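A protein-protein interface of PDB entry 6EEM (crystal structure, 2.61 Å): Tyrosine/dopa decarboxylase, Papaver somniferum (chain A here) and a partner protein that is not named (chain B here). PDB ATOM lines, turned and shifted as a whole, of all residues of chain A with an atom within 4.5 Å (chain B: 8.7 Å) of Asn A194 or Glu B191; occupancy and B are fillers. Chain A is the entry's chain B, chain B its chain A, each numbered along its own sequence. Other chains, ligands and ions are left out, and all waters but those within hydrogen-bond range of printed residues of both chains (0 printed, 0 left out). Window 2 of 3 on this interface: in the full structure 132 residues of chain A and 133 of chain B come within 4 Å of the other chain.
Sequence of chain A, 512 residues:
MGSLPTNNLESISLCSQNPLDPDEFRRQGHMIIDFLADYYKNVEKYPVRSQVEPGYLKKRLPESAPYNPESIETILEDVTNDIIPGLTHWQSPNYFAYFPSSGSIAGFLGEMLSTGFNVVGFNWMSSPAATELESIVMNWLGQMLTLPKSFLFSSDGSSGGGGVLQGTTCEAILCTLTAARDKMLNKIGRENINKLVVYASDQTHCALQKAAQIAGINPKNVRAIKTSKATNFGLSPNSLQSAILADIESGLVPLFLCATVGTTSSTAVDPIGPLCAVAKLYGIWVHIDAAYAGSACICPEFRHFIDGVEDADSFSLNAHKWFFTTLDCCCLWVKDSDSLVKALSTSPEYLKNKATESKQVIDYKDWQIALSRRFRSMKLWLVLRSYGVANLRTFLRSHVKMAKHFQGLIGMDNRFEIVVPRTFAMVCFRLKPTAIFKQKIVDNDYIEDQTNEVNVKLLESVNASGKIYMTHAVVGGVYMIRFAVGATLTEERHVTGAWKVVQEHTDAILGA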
ATOM      1  N   ASN A 192      17.413 -19.722 -12.249  1.00  0.00           N
ATOM      2  CA  ASN A 192      18.037 -20.878 -12.878  1.00  0.00           C
ATOM      3  C   ASN A 192      18.896 -20.504 -14.085  1.00  0.00           C
ATOM      4  O   ASN A 192      19.339 -21.397 -14.814  1.00  0.00           O
ATOM      5  CB  ASN A 192      16.970 -21.897 -13.303  1.00  0.00           C
ATOM      6  CG  ASN A 192      16.216 -22.500 -12.119  1.00  0.00           C
ATOM      7  OD1 ASN A 192      16.768 -23.282 -11.343  1.00  0.00           O
ATOM      8  ND2 ASN A 192      14.942 -22.155 -11.995  1.00  0.00           N
ATOM      9  N   ILE A 193      19.151 -19.213 -14.316  1.00  0.00           N
ATOM     10  CA  ILE A 193      19.866 -18.819 -15.529  1.00  0.00           C
ATOM     11  C   ILE A 193      21.250 -19.454 -15.575  1.00  0.00           C
ATOM     12  O   ILE A 193      21.728 -19.856 -16.641  1.00  0.00           O
ATOM     13  CB  ILE A 193      19.948 -17.288 -15.635  1.00  0.00           C
ATOM     14  CG1 ILE A 193      20.627 -16.900 -16.950  1.00  0.00           C
ATOM     15  CG2 ILE A 193      20.694 -16.717 -14.440  1.00  0.00           C
ATOM     16  CD1 ILE A 193      20.594 -15.418 -17.249  1.00  0.00           C
ATOM     17  N   ASN A 194      21.924 -19.543 -14.430  1.00  0.00           N
ATOM     18  CA  ASN A 194      23.259 -20.127 -14.393  1.00  0.00           C
ATOM     19  C   ASN A 194      23.246 -21.650 -14.390  1.00  0.00           C
ATOM     20  O   ASN A 194      24.317 -22.260 -14.303  1.00  0.00           O
ATOM     21  CB  ASN A 194      24.031 -19.605 -13.177  1.00  0.00           C
ATOM     22  CG  ASN A 194      24.595 -18.211 -13.404  1.00  0.00           C
ATOM     23  OD1 ASN A 194      25.246 -17.957 -14.417  1.00  0.00           O
ATOM     24  ND2 ASN A 194      24.329 -17.294 -12.470  1.00  0.00           N
ATOM     25  N   LYS A 195      22.077 -22.278 -14.489  1.00  0.00           N
ATOM     26  CA  LYS A 195      21.982 -23.723 -14.629  1.00  0.00           C
ATOM     27  C   LYS A 195      21.631 -24.147 -16.047  1.00  0.00           C
ATOM     28  O   LYS A 195      21.588 -25.346 -16.327  1.00  0.00           O
ATOM     29  CB  LYS A 195      20.949 -24.286 -13.645  1.00  0.00           C
ATOM     30  CG  LYS A 195      21.329 -24.068 -12.188  1.00  0.00           C
ATOM     31  CD  LYS A 195      20.288 -24.619 -11.223  1.00  0.00           C
ATOM     32  CE  LYS A 195      20.795 -24.538  -9.788  1.00  0.00           C
ATOM     33  NZ  LYS A 195      19.863 -25.175  -8.809  1.00  0.00           N
ATOM     34  N   LEU A 196      21.378 -23.192 -16.940  1.00  0.00           N
ATOM     35  CA  LEU A 196      21.006 -23.508 -18.310  1.00  0.00           C
ATOM     36  C   LEU A 196      22.218 -24.006 -19.085  1.00  0.00           C
ATOM     37  O   LEU A 196      23.314 -23.448 -18.977  1.00  0.00           O
ATOM     38  CB  LEU A 196      20.413 -22.277 -18.993  1.00  0.00           C
ATOM     39  CG  LEU A 196      19.198 -21.657 -18.305  1.00  0.00           C
ATOM     40  CD1 LEU A 196      18.781 -20.388 -19.023  1.00  0.00           C
ATOM     41  CD2 LEU A 196      18.045 -22.643 -18.259  1.00  0.00           C
ATOM     42  N   GLY A 216      24.084 -14.566 -21.564  1.00  0.00           N
ATOM     43  CA  GLY A 216      24.204 -14.791 -20.142  1.00  0.00           C
ATOM     44  C   GLY A 216      24.287 -16.237 -19.713  1.00  0.00           C
ATOM     45  O   GLY A 216      24.226 -16.510 -18.508  1.00  0.00           O
ATOM     46  N   ASN A 218      26.057 -19.404 -18.511  1.00  0.00           N
ATOM     47  CA  ASN A 218      27.316 -19.548 -17.793  1.00  0.00           C
ATOM     48  C   ASN A 218      28.327 -20.284 -18.670  1.00  0.00           C
ATOM     49  O   ASN A 218      28.000 -21.338 -19.231  1.00  0.00           O
ATOM     50  CB  ASN A 218      27.120 -20.298 -16.479  1.00  0.00           C
ATOM     51  CG  ASN A 218      28.382 -20.328 -15.643  1.00  0.00           C
ATOM     52  OD1 ASN A 218      29.371 -20.978 -16.009  1.00  0.00           O
ATOM     53  ND2 ASN A 218      28.367 -19.612 -14.523  1.00  0.00           N
ATOM     54  N   ASN A 221      28.640 -23.994 -18.953  1.00  0.00           N
ATOM     55  CA  ASN A 221      27.470 -24.746 -19.392  1.00  0.00           C
ATOM     56  C   ASN A 221      27.301 -24.688 -20.904  1.00  0.00           C
ATOM     57  O   ASN A 221      26.190 -24.817 -21.423  1.00  0.00           O
ATOM     58  CB  ASN A 221      26.208 -24.247 -18.687  1.00  0.00           C
ATOM     59  CG  ASN A 221      26.239 -24.501 -17.194  1.00  0.00           C
ATOM     60  OD1 ASN A 221      26.842 -25.473 -16.734  1.00  0.00           O
ATOM     61  ND2 ASN A 221      25.587 -23.630 -16.426  1.00  0.00           N
ATOM     62  N   LEU B 185      30.830  -9.211 -13.140  1.00  0.00           N
ATOM     63  CA  LEU B 185      30.626 -10.582 -12.698  1.00  0.00           C
ATOM     64  C   LEU B 185      31.941 -11.329 -12.556  1.00  0.00           C
ATOM     65  O   LEU B 185      32.040 -12.239 -11.726  1.00  0.00           O
ATOM     66  CB  LEU B 185      29.684 -11.313 -13.652  1.00  0.00           C
ATOM     67  CG  LEU B 185      28.266 -10.737 -13.684  1.00  0.00           C
ATOM     68  CD1 LEU B 185      27.323 -11.583 -14.545  1.00  0.00           C
ATOM     69  CD2 LEU B 185      27.734 -10.595 -12.274  1.00  0.00           C
ATOM     70  N   ASN B 186      32.964 -10.967 -13.338  1.00  0.00           N
ATOM     71  CA  ASN B 186      34.278 -11.574 -13.142  1.00  0.00           C
ATOM     72  C   ASN B 186      34.794 -11.299 -11.743  1.00  0.00           C
ATOM     73  O   ASN B 186      35.536 -12.112 -11.182  1.00  0.00           O
ATOM     74  CB  ASN B 186      35.280 -11.057 -14.178  1.00  0.00           C
ATOM     75  CG  ASN B 186      35.115 -11.715 -15.541  1.00  0.00           C
ATOM     76  OD1 ASN B 186      34.516 -12.787 -15.664  1.00  0.00           O
ATOM     77  ND2 ASN B 186      35.657 -11.073 -16.575  1.00  0.00           N
ATOM     78  N   LYS B 187      34.400 -10.168 -11.161  1.00  0.00           N
ATOM     79  CA  LYS B 187      34.842  -9.846  -9.810  1.00  0.00           C
ATOM     80  C   LYS B 187      33.943 -10.481  -8.756  1.00  0.00           C
ATOM     81  O   LYS B 187      34.439 -11.086  -7.796  1.00  0.00           O
ATOM     82  CB  LYS B 187      34.916  -8.329  -9.628  1.00  0.00           C
ATOM     83  CG  LYS B 187      35.912  -7.658 -10.571  1.00  0.00           C
ATOM     84  CD  LYS B 187      36.175  -6.202 -10.225  1.00  0.00           C
ATOM     85  CE  LYS B 187      34.980  -5.308 -10.545  1.00  0.00           C
ATOM     86  NZ  LYS B 187      35.285  -3.873 -10.261  1.00  0.00           N
ATOM     87  N   ILE B 188      32.621 -10.389  -8.924  1.00  0.00           N
ATOM     88  CA  ILE B 188      31.725 -10.758  -7.827  1.00  0.00           C
ATOM     89  C   ILE B 188      31.040 -12.112  -8.011  1.00  0.00           C
ATOM     90  O   ILE B 188      30.377 -12.579  -7.071  1.00  0.00           O
ATOM     91  CB  ILE B 188      30.675  -9.656  -7.569  1.00  0.00           C
ATOM     92  CG1 ILE B 188      29.731  -9.499  -8.762  1.00  0.00           C
ATOM     93  CG2 ILE B 188      31.375  -8.348  -7.252  1.00  0.00           C
ATOM     94  CD1 ILE B 188      28.586  -8.494  -8.512  1.00  0.00           C
ATOM     95  N   GLY B 189      31.192 -12.765  -9.165  1.00  0.00           N
ATOM     96  CA  GLY B 189      30.567 -14.058  -9.375  1.00  0.00           C
ATOM     97  C   GLY B 189      29.286 -14.004 -10.184  1.00  0.00           C
ATOM     98  O   GLY B 189      28.409 -13.176  -9.913  1.00  0.00           O
ATOM     99  N   ARG B 190      29.147 -14.902 -11.166  1.00  0.00           N
ATOM    100  CA  ARG B 190      27.991 -14.856 -12.056  1.00  0.00           C
ATOM    101  C   ARG B 190      26.672 -15.076 -11.325  1.00  0.00           C
ATOM    102  O   ARG B 190      25.618 -14.702 -11.851  1.00  0.00           O
ATOM    103  CB  ARG B 190      28.135 -15.891 -13.173  1.00  0.00           C
ATOM    104  CG  ARG B 190      29.406 -15.756 -13.987  1.00  0.00           C
ATOM    105  CD  ARG B 190      29.142 -15.755 -15.482  1.00  0.00           C
ATOM    106  NE  ARG B 190      30.391 -15.903 -16.231  1.00  0.00           N
ATOM    107  CZ  ARG B 190      31.269 -14.925 -16.442  1.00  0.00           C
ATOM    108  NH1 ARG B 190      31.043 -13.707 -15.963  1.00  0.00           N
ATOM    109  NH2 ARG B 190      32.380 -15.163 -17.132  1.00  0.00           N
ATOM    110  N   GLU B 191      26.693 -15.678 -10.135  1.00  0.00           N
ATOM    111  CA  GLU B 191      25.454 -15.870  -9.398  1.00  0.00           C
ATOM    112  C   GLU B 191      24.746 -14.545  -9.116  1.00  0.00           C
ATOM    113  O   GLU B 191      23.547 -14.547  -8.811  1.00  0.00           O
ATOM    114  CB  GLU B 191      25.727 -16.626  -8.092  1.00  0.00           C
ATOM    115  CG  GLU B 191      26.427 -15.808  -7.005  1.00  0.00           C
ATOM    116  CD  GLU B 191      27.938 -16.038  -6.942  1.00  0.00           C
ATOM    117  OE1 GLU B 191      28.493 -16.005  -5.816  1.00  0.00           O
ATOM    118  OE2 GLU B 191      28.567 -16.245  -8.009  1.00  0.00           O
ATOM    119  N   ASN B 192      25.452 -13.416  -9.228  1.00  0.00           N
ATOM    120  CA  ASN B 192      24.873 -12.094  -9.014  1.00  0.00           C
ATOM    121  C   ASN B 192      24.229 -11.496 -10.267  1.00  0.00           C
ATOM    122  O   ASN B 192      23.812 -10.334 -10.237  1.00  0.00           O
ATOM    123  CB  ASN B 192      25.939 -11.132  -8.479  1.00  0.00           C
ATOM    124  CG  ASN B 192      26.314 -11.427  -7.039  1.00  0.00           C
ATOM    125  OD1 ASN B 192      25.542 -11.148  -6.119  1.00  0.00           O
ATOM    126  ND2 ASN B 192      27.500 -11.995  -6.831  1.00  0.00           N
ATOM    127  N   ILE B 193      24.119 -12.255 -11.359  1.00  0.00           N
ATOM    128  CA  ILE B 193      23.577 -11.683 -12.587  1.00  0.00           C
ATOM    129  C   ILE B 193      22.188 -11.099 -12.358  1.00  0.00           C
ATOM    130  O   ILE B 193      21.815 -10.101 -12.989  1.00  0.00           O
ATOM    131  CB  ILE B 193      23.569 -12.740 -13.710  1.00  0.00           C
ATOM    132  CG1 ILE B 193      23.123 -12.112 -15.028  1.00  0.00           C
ATOM    133  CG2 ILE B 193      22.672 -13.892 -13.349  1.00  0.00           C
ATOM    134  CD1 ILE B 193      23.464 -12.939 -16.227  1.00  0.00           C
ATOM    135  N   ASN B 194      21.403 -11.696 -11.462  1.00  0.00           N
ATOM    136  CA  ASN B 194      20.035 -11.236 -11.249  1.00  0.00           C
ATOM    137  C   ASN B 194      19.941 -10.054 -10.297  1.00  0.00           C
ATOM    138  O   ASN B 194      18.833  -9.580 -10.036  1.00  0.00           O
ATOM    139  CB  ASN B 194      19.159 -12.386 -10.746  1.00  0.00           C
ATOM    140  CG  ASN B 194      18.611 -13.229 -11.884  1.00  0.00           C
ATOM    141  OD1 ASN B 194      18.058 -12.695 -12.850  1.00  0.00           O
ATOM    142  ND2 ASN B 194      18.782 -14.541 -11.793  1.00  0.00           N
ATOM    143  N   LYS B 195      21.065  -9.559  -9.789  1.00  0.00           N
ATOM    144  CA  LYS B 195      21.081  -8.376  -8.945  1.00  0.00           C
ATOM    145  C   LYS B 195      21.692  -7.168  -9.642  1.00  0.00           C
ATOM    146  O   LYS B 195      21.702  -6.075  -9.064  1.00  0.00           O
ATOM    147  CB  LYS B 195      21.836  -8.663  -7.643  1.00  0.00           C
ATOM    148  CG  LYS B 195      21.118  -9.613  -6.693  1.00  0.00           C
ATOM    149  CD  LYS B 195      21.997  -9.931  -5.484  1.00  0.00           C
ATOM    150  CE  LYS B 195      21.327 -10.893  -4.523  1.00  0.00           C
ATOM    151  NZ  LYS B 195      22.365 -11.674  -3.782  1.00  0.00           N
ATOM    152  N   LEU B 196      22.196  -7.335 -10.865  1.00  0.00           N
ATOM    153  CA  LEU B 196      22.747  -6.213 -11.613  1.00  0.00           C
ATOM    154  C   LEU B 196      21.633  -5.253 -12.027  1.00  0.00           C
ATOM    155  O   LEU B 196      20.582  -5.677 -12.515  1.00  0.00           O
ATOM    156  CB  LEU B 196      23.502  -6.731 -12.836  1.00  0.00           C
ATOM    157  CG  LEU B 196      24.589  -7.759 -12.507  1.00  0.00           C
ATOM    158  CD1 LEU B 196      25.207  -8.349 -13.768  1.00  0.00           C
ATOM    159  CD2 LEU B 196      25.662  -7.132 -11.628  1.00  0.00           C
ATOM    160  N   VAL B 253      23.158  -4.614  -7.137  1.00  0.00           N
ATOM    161  CA  VAL B 253      24.480  -4.291  -7.658  1.00  0.00           C
ATOM    162  C   VAL B 253      24.318  -3.313  -8.813  1.00  0.00           C
ATOM    163  O   VAL B 253      24.043  -3.714  -9.945  1.00  0.00           O
ATOM    164  CB  VAL B 253      25.228  -5.555  -8.116  1.00  0.00           C
ATOM    165  CG1 VAL B 253      26.620  -5.195  -8.575  1.00  0.00           C
ATOM    166  CG2 VAL B 253      25.260  -6.590  -7.013  1.00  0.00           C
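The backbone carbonyl oxygen (O) of Arg B190 is in hydrogen-bond range of the side-chain amide nitrogen (ND2) of Asn A194 (3.0 Å).
Of the 13 printed residues of chain B, 4 touch a printed residue of chain A. Hydrophobic or aromatic side chains of chain B within 4 Å of the printed part of chain A: Ile B193. Hydrophobic or aromatic side chains of chain A within 4 Å of the printed part of chain B: Ile A193. Along chain A the printed residues that touch a printed residue of chain B span positions 193 to 218. Among the printed residues, no Asp or Glu carboxylate lies within 4 Å of a Lys or Arg side-chain nitrogen of the other chain.
Ile A193 touches Ile B193 (CG2 to CG2, 3.6 Å). Asn B194 touches Ile A193. Asn A194 touches Glu B191. Asn A194 touches Ile B193. Asn A218 touches Arg B190.
The backbone carbonyl oxygen of Asn A194 lies within hydrogen-bond range of the side-chain amide nitrogen of Asn A221.
Of the printed residues of chain B, Ile A193 touches Ile B193 (3.6 Å) and Asn B194 (3.9 Å). Of chain B, only Arg B190 (3.0 Å), Glu B191 (3.6 Å) and Ile B193 (3.9 Å) come within 4 Å of Asn A194. Of the printed residues of chain B, Asn A218 touches Arg B190. Of the printed residues of chain A, Arg B190 touches Asn A194 and Asn A218. Of chain A, only Asn A194 (3.6 Å) comes within 4 Å of Glu B191. Lys B195 touches none of the printed residues of chain A. The nearest printed residue of chain A that does not touch Glu B191 is Asn A218 (6.1 Å).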
